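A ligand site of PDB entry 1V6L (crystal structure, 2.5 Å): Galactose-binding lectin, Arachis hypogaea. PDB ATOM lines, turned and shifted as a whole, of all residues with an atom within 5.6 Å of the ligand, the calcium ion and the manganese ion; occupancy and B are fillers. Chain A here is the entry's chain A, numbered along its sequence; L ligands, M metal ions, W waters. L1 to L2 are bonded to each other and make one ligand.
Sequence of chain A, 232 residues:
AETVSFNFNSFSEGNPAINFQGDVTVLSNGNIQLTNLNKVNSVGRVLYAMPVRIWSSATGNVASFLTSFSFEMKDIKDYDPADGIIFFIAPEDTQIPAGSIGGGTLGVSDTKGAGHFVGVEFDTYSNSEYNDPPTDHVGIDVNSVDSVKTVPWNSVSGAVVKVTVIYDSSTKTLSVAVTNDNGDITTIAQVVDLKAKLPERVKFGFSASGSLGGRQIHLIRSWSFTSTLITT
Water W4 lies within hydrogen-bond range of the backbone carbonyl oxygen (O) of Val 145 and the side-chain carboxylate (OE1) of Glu 121. Water W3 lies within hydrogen-bond range of O1 of LG2 L2 (2.7 Å) and N of Gly 104 (3.0 Å). Water W8 lies within hydrogen-bond range of the side-chain carboxylate of Glu 129 (2.8 Å), an oxygen (O1) of LG2 L2 (3.0 Å) and the side-chain amide nitrogen of Asn 127 (3.2 Å).
The manganese ion is bound by the side-chain carboxylate of Glu 121 (2.2 Å), the side-chain carboxylate of Asp 132 (2.2 Å), water W7 (2.2 Å), the side-chain carboxylate of Asp 123 (2.3 Å), a ring nitrogen (NE2) of His 137 (2.3 Å) and water W4 (2.4 Å).
O2 of LG2 L2 is in hydrogen-bond range of ND2 of Asn 127. N of Gly 104 lies within hydrogen-bond range of O2 of LG2 L2 (2.9 Å). OD1 of Asp 83 is in hydrogen-bond range of O2 of LG2 L2 (2.7 Å). O3 of LG2 L2 is in hydrogen-bond range of OG of Ser 211 (2.8 Å). An oxygen (O3) of LIG L1 is in hydrogen-bond range of the backbone NH of Gly 213.
Asp 80 touches the ligand. Gly 103 touches the ligand. CD2 of Leu 212 touches O2 of LIG L1, at 3.6 Å. Gly 214 touches the ligand. Within 4 Å of the ligand: Asp 80, Asp 83, Gly 103, Gly 104, Tyr 125, Asn 127, Ser 211, Leu 212, Gly 213 and Gly 214. The nearest printed residue that does not touch the ligand is Ala 82 (4.02 Å).
Along chain A the residues within 4 Å of the calcium ion span positions 123 to 132. The nearest printed residue that does not touch the calcium ion is Gly 104 (4.2 Å).
The calcium ion is bound by OD2 of Asp 132. The side-chain amide oxygen (OD1) of Asn 127 binds the calcium ion (2.6 Å). The calcium ion is bound by O of Tyr 125. The calcium ion is bound by water W1, 2.6 Å away. OD1 of Asp 123 binds the calcium ion (2.7 Å). Water W2 binds the calcium ion (2.7 Å). OD2 of Asp 123 binds the calcium ion.
The backbone carbonyl oxygen (O) of Gly 213 sits at hydrogen-bond distance from the backbone NH (N) of Asp 80 (3.0 Å). The side-chain amide nitrogen (ND2) of Asn 127 lies within hydrogen-bond range of the side-chain carboxylate (OE2) of Glu 129. N of Gly 214 lies within hydrogen-bond range of OG of Ser 211. N of Gly 103 is in hydrogen-bond range of O of Gly 210 (2.8 Å). The backbone carbonyl oxygen (O) of Asp 83 is in hydrogen-bond range of the side-chain hydroxyl (OG1) of Thr 124 (2.4 Å).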
ATOM      1  N   ASP A  80     -36.994 -17.017  14.776  1.00  0.00           N
ATOM      2  CA  ASP A  80     -35.686 -16.548  14.318  1.00  0.00           C
ATOM      3  C   ASP A  80     -35.480 -17.061  12.900  1.00  0.00           C
ATOM      4  O   ASP A  80     -36.066 -18.050  12.501  1.00  0.00           O
ATOM      5  CB  ASP A  80     -34.540 -17.088  15.171  1.00  0.00           C
ATOM      6  CG  ASP A  80     -34.255 -16.235  16.377  1.00  0.00           C
ATOM      7  OD1 ASP A  80     -35.184 -16.003  17.168  1.00  0.00           O
ATOM      8  OD2 ASP A  80     -33.089 -15.795  16.533  1.00  0.00           O
ATOM      9  N   ALA A  82     -32.132 -17.680  10.339  1.00  0.00           N
ATOM     10  CA  ALA A  82     -32.366 -19.067  10.736  1.00  0.00           C
ATOM     11  C   ALA A  82     -33.009 -19.973   9.665  1.00  0.00           C
ATOM     12  O   ALA A  82     -34.215 -19.898   9.380  1.00  0.00           O
ATOM     13  CB  ALA A  82     -33.158 -19.142  12.071  1.00  0.00           C
ATOM     14  N   ASP A  83     -32.201 -20.828   9.048  1.00  0.00           N
ATOM     15  CA  ASP A  83     -30.752 -20.917   9.296  1.00  0.00           C
ATOM     16  C   ASP A  83     -30.081 -20.421   8.005  1.00  0.00           C
ATOM     17  O   ASP A  83     -29.179 -19.577   8.022  1.00  0.00           O
ATOM     18  CB  ASP A  83     -30.371 -22.368   9.638  1.00  0.00           C
ATOM     19  CG  ASP A  83     -30.506 -22.660  11.124  1.00  0.00           C
ATOM     20  OD1 ASP A  83     -29.619 -22.238  11.890  1.00  0.00           O
ATOM     21  OD2 ASP A  83     -31.490 -23.310  11.539  1.00  0.00           O
ATOM     22  N   GLY A 102     -30.582 -30.488  11.767  1.00  0.00           N
ATOM     23  CA  GLY A 102     -30.884 -29.309  10.981  1.00  0.00           C
ATOM     24  C   GLY A 102     -30.107 -28.131  11.533  1.00  0.00           C
ATOM     25  O   GLY A 102     -28.909 -28.246  11.784  1.00  0.00           O
ATOM     26  N   GLY A 103     -30.780 -27.005  11.731  1.00  0.00           N
ATOM     27  CA  GLY A 103     -30.117 -25.824  12.276  1.00  0.00           C
ATOM     28  C   GLY A 103     -28.833 -25.479  11.546  1.00  0.00           C
ATOM     29  O   GLY A 103     -28.787 -25.466  10.315  1.00  0.00           O
ATOM     30  N   GLY A 104     -27.777 -25.205  12.316  1.00  0.00           N
ATOM     31  CA  GLY A 104     -26.494 -24.849  11.751  1.00  0.00           C
ATOM     32  C   GLY A 104     -25.855 -25.836  10.801  1.00  0.00           C
ATOM     33  O   GLY A 104     -25.003 -25.455   9.995  1.00  0.00           O
ATOM     34  N   LEU A 106     -27.114 -27.087   8.329  1.00  0.00           N
ATOM     35  CA  LEU A 106     -27.600 -26.774   6.987  1.00  0.00           C
ATOM     36  C   LEU A 106     -28.061 -28.002   6.202  1.00  0.00           C
ATOM     37  O   LEU A 106     -28.235 -27.944   4.990  1.00  0.00           O
ATOM     38  CB  LEU A 106     -26.531 -26.024   6.183  1.00  0.00           C
ATOM     39  CG  LEU A 106     -26.081 -24.683   6.788  1.00  0.00           C
ATOM     40  CD1 LEU A 106     -25.030 -24.044   5.885  1.00  0.00           C
ATOM     41  CD2 LEU A 106     -27.275 -23.758   6.929  1.00  0.00           C
ATOM     42  N   GLU A 121     -22.388 -21.511   1.001  1.00  0.00           N
ATOM     43  CA  GLU A 121     -23.473 -21.250   1.939  1.00  0.00           C
ATOM     44  C   GLU A 121     -23.881 -19.797   2.109  1.00  0.00           C
ATOM     45  O   GLU A 121     -23.074 -18.874   2.034  1.00  0.00           O
ATOM     46  CB  GLU A 121     -23.114 -21.808   3.310  1.00  0.00           C
ATOM     47  CG  GLU A 121     -21.922 -21.125   3.949  1.00  0.00           C
ATOM     48  CD  GLU A 121     -21.747 -21.513   5.391  1.00  0.00           C
ATOM     49  OE1 GLU A 121     -21.642 -22.718   5.684  1.00  0.00           O
ATOM     50  OE2 GLU A 121     -21.716 -20.605   6.242  1.00  0.00           O
ATOM     51  N   ASP A 123     -25.505 -18.342   4.954  1.00  0.00           N
ATOM     52  CA  ASP A 123     -25.798 -18.526   6.369  1.00  0.00           C
ATOM     53  C   ASP A 123     -26.417 -17.306   7.031  1.00  0.00           C
ATOM     54  O   ASP A 123     -25.837 -16.220   7.014  1.00  0.00           O
ATOM     55  CB  ASP A 123     -24.500 -18.877   7.064  1.00  0.00           C
ATOM     56  CG  ASP A 123     -24.721 -19.688   8.280  1.00  0.00           C
ATOM     57  OD1 ASP A 123     -25.731 -19.446   8.988  1.00  0.00           O
ATOM     58  OD2 ASP A 123     -23.887 -20.567   8.553  1.00  0.00           O
ATOM     59  N   THR A 124     -27.585 -17.492   7.659  1.00  0.00           N
ATOM     60  CA  THR A 124     -28.287 -16.394   8.297  1.00  0.00           C
ATOM     61  C   THR A 124     -28.313 -16.412   9.818  1.00  0.00           C
ATOM     62  O   THR A 124     -28.923 -15.544  10.446  1.00  0.00           O
ATOM     63  CB  THR A 124     -29.746 -16.319   7.811  1.00  0.00           C
ATOM     64  OG1 THR A 124     -30.440 -17.509   8.217  1.00  0.00           O
ATOM     65  CG2 THR A 124     -29.780 -16.187   6.295  1.00  0.00           C
ATOM     66  N   TYR A 125     -27.656 -17.387  10.423  1.00  0.00           N
ATOM     67  CA  TYR A 125     -27.585 -17.466  11.861  1.00  0.00           C
ATOM     68  C   TYR A 125     -26.145 -17.758  12.267  1.00  0.00           C
ATOM     69  O   TYR A 125     -25.435 -18.467  11.552  1.00  0.00           O
ATOM     70  CB  TYR A 125     -28.508 -18.548  12.415  1.00  0.00           C
ATOM     71  CG  TYR A 125     -28.482 -18.614  13.918  1.00  0.00           C
ATOM     72  CD1 TYR A 125     -27.529 -19.382  14.589  1.00  0.00           C
ATOM     73  CD2 TYR A 125     -29.363 -17.843  14.686  1.00  0.00           C
ATOM     74  CE1 TYR A 125     -27.453 -19.382  15.983  1.00  0.00           C
ATOM     75  CE2 TYR A 125     -29.298 -17.832  16.072  1.00  0.00           C
ATOM     76  CZ  TYR A 125     -28.342 -18.605  16.715  1.00  0.00           C
ATOM     77  OH  TYR A 125     -28.263 -18.603  18.091  1.00  0.00           O
ATOM     78  N   SER A 126     -25.706 -17.217  13.391  1.00  0.00           N
ATOM     79  CA  SER A 126     -24.333 -17.421  13.816  1.00  0.00           C
ATOM     80  C   SER A 126     -24.129 -18.551  14.831  1.00  0.00           C
ATOM     81  O   SER A 126     -24.311 -18.365  16.038  1.00  0.00           O
ATOM     82  CB  SER A 126     -23.798 -16.092  14.375  1.00  0.00           C
ATOM     83  OG  SER A 126     -22.409 -16.158  14.615  1.00  0.00           O
ATOM     84  N   ASN A 127     -23.754 -19.730  14.337  1.00  0.00           N
ATOM     85  CA  ASN A 127     -23.511 -20.880  15.210  1.00  0.00           C
ATOM     86  C   ASN A 127     -22.071 -20.879  15.676  1.00  0.00           C
ATOM     87  O   ASN A 127     -21.167 -21.227  14.917  1.00  0.00           O
ATOM     88  CB  ASN A 127     -23.776 -22.188  14.481  1.00  0.00           C
ATOM     89  CG  ASN A 127     -25.241 -22.414  14.210  1.00  0.00           C
ATOM     90  OD1 ASN A 127     -25.809 -21.800  13.319  1.00  0.00           O
ATOM     91  ND2 ASN A 127     -25.865 -23.298  14.982  1.00  0.00           N
ATOM     92  N   GLU A 129     -20.665 -22.869  17.608  1.00  0.00           N
ATOM     93  CA  GLU A 129     -20.114 -24.226  17.611  1.00  0.00           C
ATOM     94  C   GLU A 129     -19.402 -24.544  16.294  1.00  0.00           C
ATOM     95  O   GLU A 129     -18.608 -25.477  16.244  1.00  0.00           O
ATOM     96  CB  GLU A 129     -21.214 -25.255  17.863  1.00  0.00           C
ATOM     97  CG  GLU A 129     -22.308 -25.288  16.812  1.00  0.00           C
ATOM     98  CD  GLU A 129     -23.521 -24.444  17.178  1.00  0.00           C
ATOM     99  OE1 GLU A 129     -23.335 -23.304  17.657  1.00  0.00           O
ATOM    100  OE2 GLU A 129     -24.656 -24.925  16.965  1.00  0.00           O
ATOM    101  N   TYR A 130     -19.694 -23.771  15.252  1.00  0.00           N
ATOM    102  CA  TYR A 130     -19.063 -23.999  13.953  1.00  0.00           C
ATOM    103  C   TYR A 130     -18.226 -22.794  13.536  1.00  0.00           C
ATOM    104  O   TYR A 130     -17.874 -22.638  12.369  1.00  0.00           O
ATOM    105  CB  TYR A 130     -20.126 -24.285  12.887  1.00  0.00           C
ATOM    106  CG  TYR A 130     -21.057 -25.418  13.240  1.00  0.00           C
ATOM    107  CD1 TYR A 130     -20.565 -26.669  13.612  1.00  0.00           C
ATOM    108  CD2 TYR A 130     -22.446 -25.236  13.228  1.00  0.00           C
ATOM    109  CE1 TYR A 130     -21.436 -27.720  13.954  1.00  0.00           C
ATOM    110  CE2 TYR A 130     -23.312 -26.269  13.560  1.00  0.00           C
ATOM    111  CZ  TYR A 130     -22.796 -27.504  13.931  1.00  0.00           C
ATOM    112  OH  TYR A 130     -23.663 -28.516  14.300  1.00  0.00           O
ATOM    113  N   ASP A 132     -18.918 -19.579  13.189  1.00  0.00           N
ATOM    114  CA  ASP A 132     -19.499 -18.644  12.236  1.00  0.00           C
ATOM    115  C   ASP A 132     -19.096 -17.216  12.534  1.00  0.00           C
ATOM    116  O   ASP A 132     -18.822 -16.857  13.674  1.00  0.00           O
ATOM    117  CB  ASP A 132     -21.027 -18.666  12.276  1.00  0.00           C
ATOM    118  CG  ASP A 132     -21.622 -19.810  11.517  1.00  0.00           C
ATOM    119  OD1 ASP A 132     -21.037 -20.219  10.500  1.00  0.00           O
ATOM    120  OD2 ASP A 132     -22.704 -20.269  11.931  1.00  0.00           O
ATOM    121  N   PRO A 133     -19.047 -16.368  11.491  1.00  0.00           N
ATOM    122  CA  PRO A 133     -18.687 -14.977  11.745  1.00  0.00           C
ATOM    123  C   PRO A 133     -19.870 -14.455  12.576  1.00  0.00           C
ATOM    124  O   PRO A 133     -20.859 -15.162  12.762  1.00  0.00           O
ATOM    125  CB  PRO A 133     -18.670 -14.368  10.347  1.00  0.00           C
ATOM    126  CG  PRO A 133     -18.236 -15.532   9.489  1.00  0.00           C
ATOM    127  CD  PRO A 133     -19.020 -16.683  10.048  1.00  0.00           C
ATOM    128  N   HIS A 137     -23.605 -14.261   6.372  1.00  0.00           N
ATOM    129  CA  HIS A 137     -22.435 -14.372   5.531  1.00  0.00           C
ATOM    130  C   HIS A 137     -22.534 -15.421   4.440  1.00  0.00           C
ATOM    131  O   HIS A 137     -23.441 -16.252   4.424  1.00  0.00           O
ATOM    132  CB  HIS A 137     -21.236 -14.711   6.410  1.00  0.00           C
ATOM    133  CG  HIS A 137     -21.435 -15.965   7.205  1.00  0.00           C
ATOM    134  ND1 HIS A 137     -22.251 -16.007   8.316  1.00  0.00           N
ATOM    135  CD2 HIS A 137     -20.954 -17.216   7.029  1.00  0.00           C
ATOM    136  CE1 HIS A 137     -22.274 -17.241   8.791  1.00  0.00           C
ATOM    137  NE2 HIS A 137     -21.485 -17.995   8.032  1.00  0.00           N
ATOM    138  N   VAL A 145     -19.141 -27.294   7.866  1.00  0.00           N
ATOM    139  CA  VAL A 145     -19.921 -26.045   7.857  1.00  0.00           C
ATOM    140  C   VAL A 145     -19.078 -24.996   8.545  1.00  0.00           C
ATOM    141  O   VAL A 145     -19.502 -23.852   8.745  1.00  0.00           O
ATOM    142  CB  VAL A 145     -21.265 -26.201   8.581  1.00  0.00           C
ATOM    143  CG1 VAL A 145     -22.187 -27.042   7.745  1.00  0.00           C
ATOM    144  CG2 VAL A 145     -21.040 -26.817   9.954  1.00  0.00           C
ATOM    145  N   SER A 147     -16.696 -23.066   7.650  1.00  0.00           N
ATOM    146  CA  SER A 147     -16.150 -22.527   6.418  1.00  0.00           C
ATOM    147  C   SER A 147     -14.647 -22.302   6.349  1.00  0.00           C
ATOM    148  O   SER A 147     -14.021 -21.838   7.297  1.00  0.00           O
ATOM    149  CB  SER A 147     -16.871 -21.234   6.076  1.00  0.00           C
ATOM    150  OG  SER A 147     -18.267 -21.446   6.029  1.00  0.00           O
ATOM    151  N   THR A 150     -15.096 -17.112   4.709  1.00  0.00           N
ATOM    152  CA  THR A 150     -16.398 -16.459   4.716  1.00  0.00           C
ATOM    153  C   THR A 150     -16.234 -14.986   4.355  1.00  0.00           C
ATOM    154  O   THR A 150     -15.129 -14.452   4.398  1.00  0.00           O
ATOM    155  CB  THR A 150     -17.079 -16.524   6.099  1.00  0.00           C
ATOM    156  OG1 THR A 150     -16.247 -15.870   7.064  1.00  0.00           O
ATOM    157  CG2 THR A 150     -17.333 -17.965   6.518  1.00  0.00           C
ATOM    158  N   GLY A 210     -33.588 -25.775   9.488  1.00  0.00           N
ATOM    159  CA  GLY A 210     -34.064 -24.895  10.533  1.00  0.00           C
ATOM    160  C   GLY A 210     -33.994 -25.658  11.844  1.00  0.00           C
ATOM    161  O   GLY A 210     -33.607 -26.820  11.865  1.00  0.00           O
ATOM    162  N   SER A 211     -34.379 -25.001  12.933  1.00  0.00           N
ATOM    163  CA  SER A 211     -34.361 -25.604  14.254  1.00  0.00           C
ATOM    164  C   SER A 211     -35.723 -25.402  14.894  1.00  0.00           C
ATOM    165  O   SER A 211     -36.704 -25.098  14.202  1.00  0.00           O
ATOM    166  CB  SER A 211     -33.267 -24.962  15.108  1.00  0.00           C
ATOM    167  OG  SER A 211     -33.442 -23.558  15.220  1.00  0.00           O
ATOM    168  N   LEU A 212     -35.809 -25.567  16.211  1.00  0.00           N
ATOM    169  CA  LEU A 212     -37.083 -25.371  16.882  1.00  0.00           C
ATOM    170  C   LEU A 212     -37.414 -23.887  16.915  1.00  0.00           C
ATOM    171  O   LEU A 212     -38.549 -23.490  16.629  1.00  0.00           O
ATOM    172  CB  LEU A 212     -37.025 -25.930  18.320  1.00  0.00           C
ATOM    173  CG  LEU A 212     -38.364 -25.963  19.055  1.00  0.00           C
ATOM    174  CD1 LEU A 212     -38.335 -27.061  20.108  1.00  0.00           C
ATOM    175  CD2 LEU A 212     -38.641 -24.607  19.680  1.00  0.00           C
ATOM    176  N   GLY A 213     -36.428 -23.071  17.255  1.00  0.00           N
ATOM    177  CA  GLY A 213     -36.648 -21.637  17.314  1.00  0.00           C
ATOM    178  C   GLY A 213     -36.315 -20.927  16.014  1.00  0.00           C
ATOM    179  O   GLY A 213     -36.853 -19.861  15.731  1.00  0.00           O
ATOM    180  N   GLY A 214     -35.415 -21.518  15.241  1.00  0.00           N
ATOM    181  CA  GLY A 214     -35.020 -20.906  13.984  1.00  0.00           C
ATOM    182  C   GLY A 214     -35.757 -21.467  12.791  1.00  0.00           C
ATOM    183  O   GLY A 214     -35.621 -22.640  12.445  1.00  0.00           O
HETATM  184  C1  LIG L   1     -33.237 -24.011  21.884  1.00  0.00           C
HETATM  185  C2  LIG L   1     -33.974 -23.386  20.684  1.00  0.00           C
HETATM  186  C3  LIG L   1     -33.292 -23.790  19.367  1.00  0.00           C
HETATM  187  C4  LIG L   1     -31.798 -23.467  19.428  1.00  0.00           C
HETATM  188  C5  LIG L   1     -31.181 -24.129  20.651  1.00  0.00           C
HETATM  189  C6  LIG L   1     -29.698 -23.818  20.809  1.00  0.00           C
HETATM  190  O1  LIG L   1     -33.333 -25.390  21.817  1.00  0.00           O
HETATM  191  O2  LIG L   1     -35.326 -23.809  20.680  1.00  0.00           O
HETATM  192  O3  LIG L   1     -33.889 -23.101  18.284  1.00  0.00           O
HETATM  193  O4  LIG L   1     -31.160 -23.935  18.227  1.00  0.00           O
HETATM  194  O5  LIG L   1     -31.842 -23.669  21.847  1.00  0.00           O
HETATM  195  O6  LIG L   1     -29.471 -22.426  20.752  1.00  0.00           O
HETATM  196  C1  LG2 L   2     -30.509 -22.973  17.460  1.00  0.00           C
HETATM  197  C2  LG2 L   2     -29.823 -23.659  16.272  1.00  0.00           C
HETATM  198  C3  LG2 L   2     -29.190 -22.602  15.351  1.00  0.00           C
HETATM  199  C4  LG2 L   2     -30.245 -21.577  14.942  1.00  0.00           C
HETATM  200  C5  LG2 L   2     -30.903 -20.973  16.186  1.00  0.00           C
HETATM  201  C6  LG2 L   2     -32.016 -20.023  15.826  1.00  0.00           C
HETATM  202  O1  LG2 L   2     -28.816 -24.552  16.725  1.00  0.00           O
HETATM  203  O2  LG2 L   2     -28.645 -23.228  14.204  1.00  0.00           O
HETATM  204  O3  LG2 L   2     -31.238 -22.212  14.146  1.00  0.00           O
HETATM  205  O4  LG2 L   2     -31.482 -22.022  16.999  1.00  0.00           O
HETATM  206  O5  LG2 L   2     -32.448 -19.271  16.955  1.00  0.00           O
HETATM  207 CA    CA M   1     -24.962 -20.982  11.010  1.00  0.00          CA
HETATM  208 MN    MN M   2     -21.641 -20.281   8.396  1.00  0.00          MN
HETATM  209  O   HOH W   1     -23.810 -23.192  10.179  1.00  0.00           O
HETATM  210  O   HOH W   2     -27.420 -21.683  10.268  1.00  0.00           O
HETATM  211  O   HOH W   3     -27.943 -26.472  15.067  1.00  0.00           O
HETATM  212  O   HOH W   4     -21.683 -22.699   8.434  1.00  0.00           O
HETATM  213  O   HOH W   5     -36.713 -21.269  21.341  1.00  0.00           O
HETATM  214  O   HOH W   6     -30.689 -26.934  18.038  1.00  0.00           O
HETATM  215  O   HOH W   7     -19.440 -20.182   8.034  1.00  0.00           O
HETATM  216  O   HOH W   8     -26.498 -23.260  18.157  1.00  0.00           O
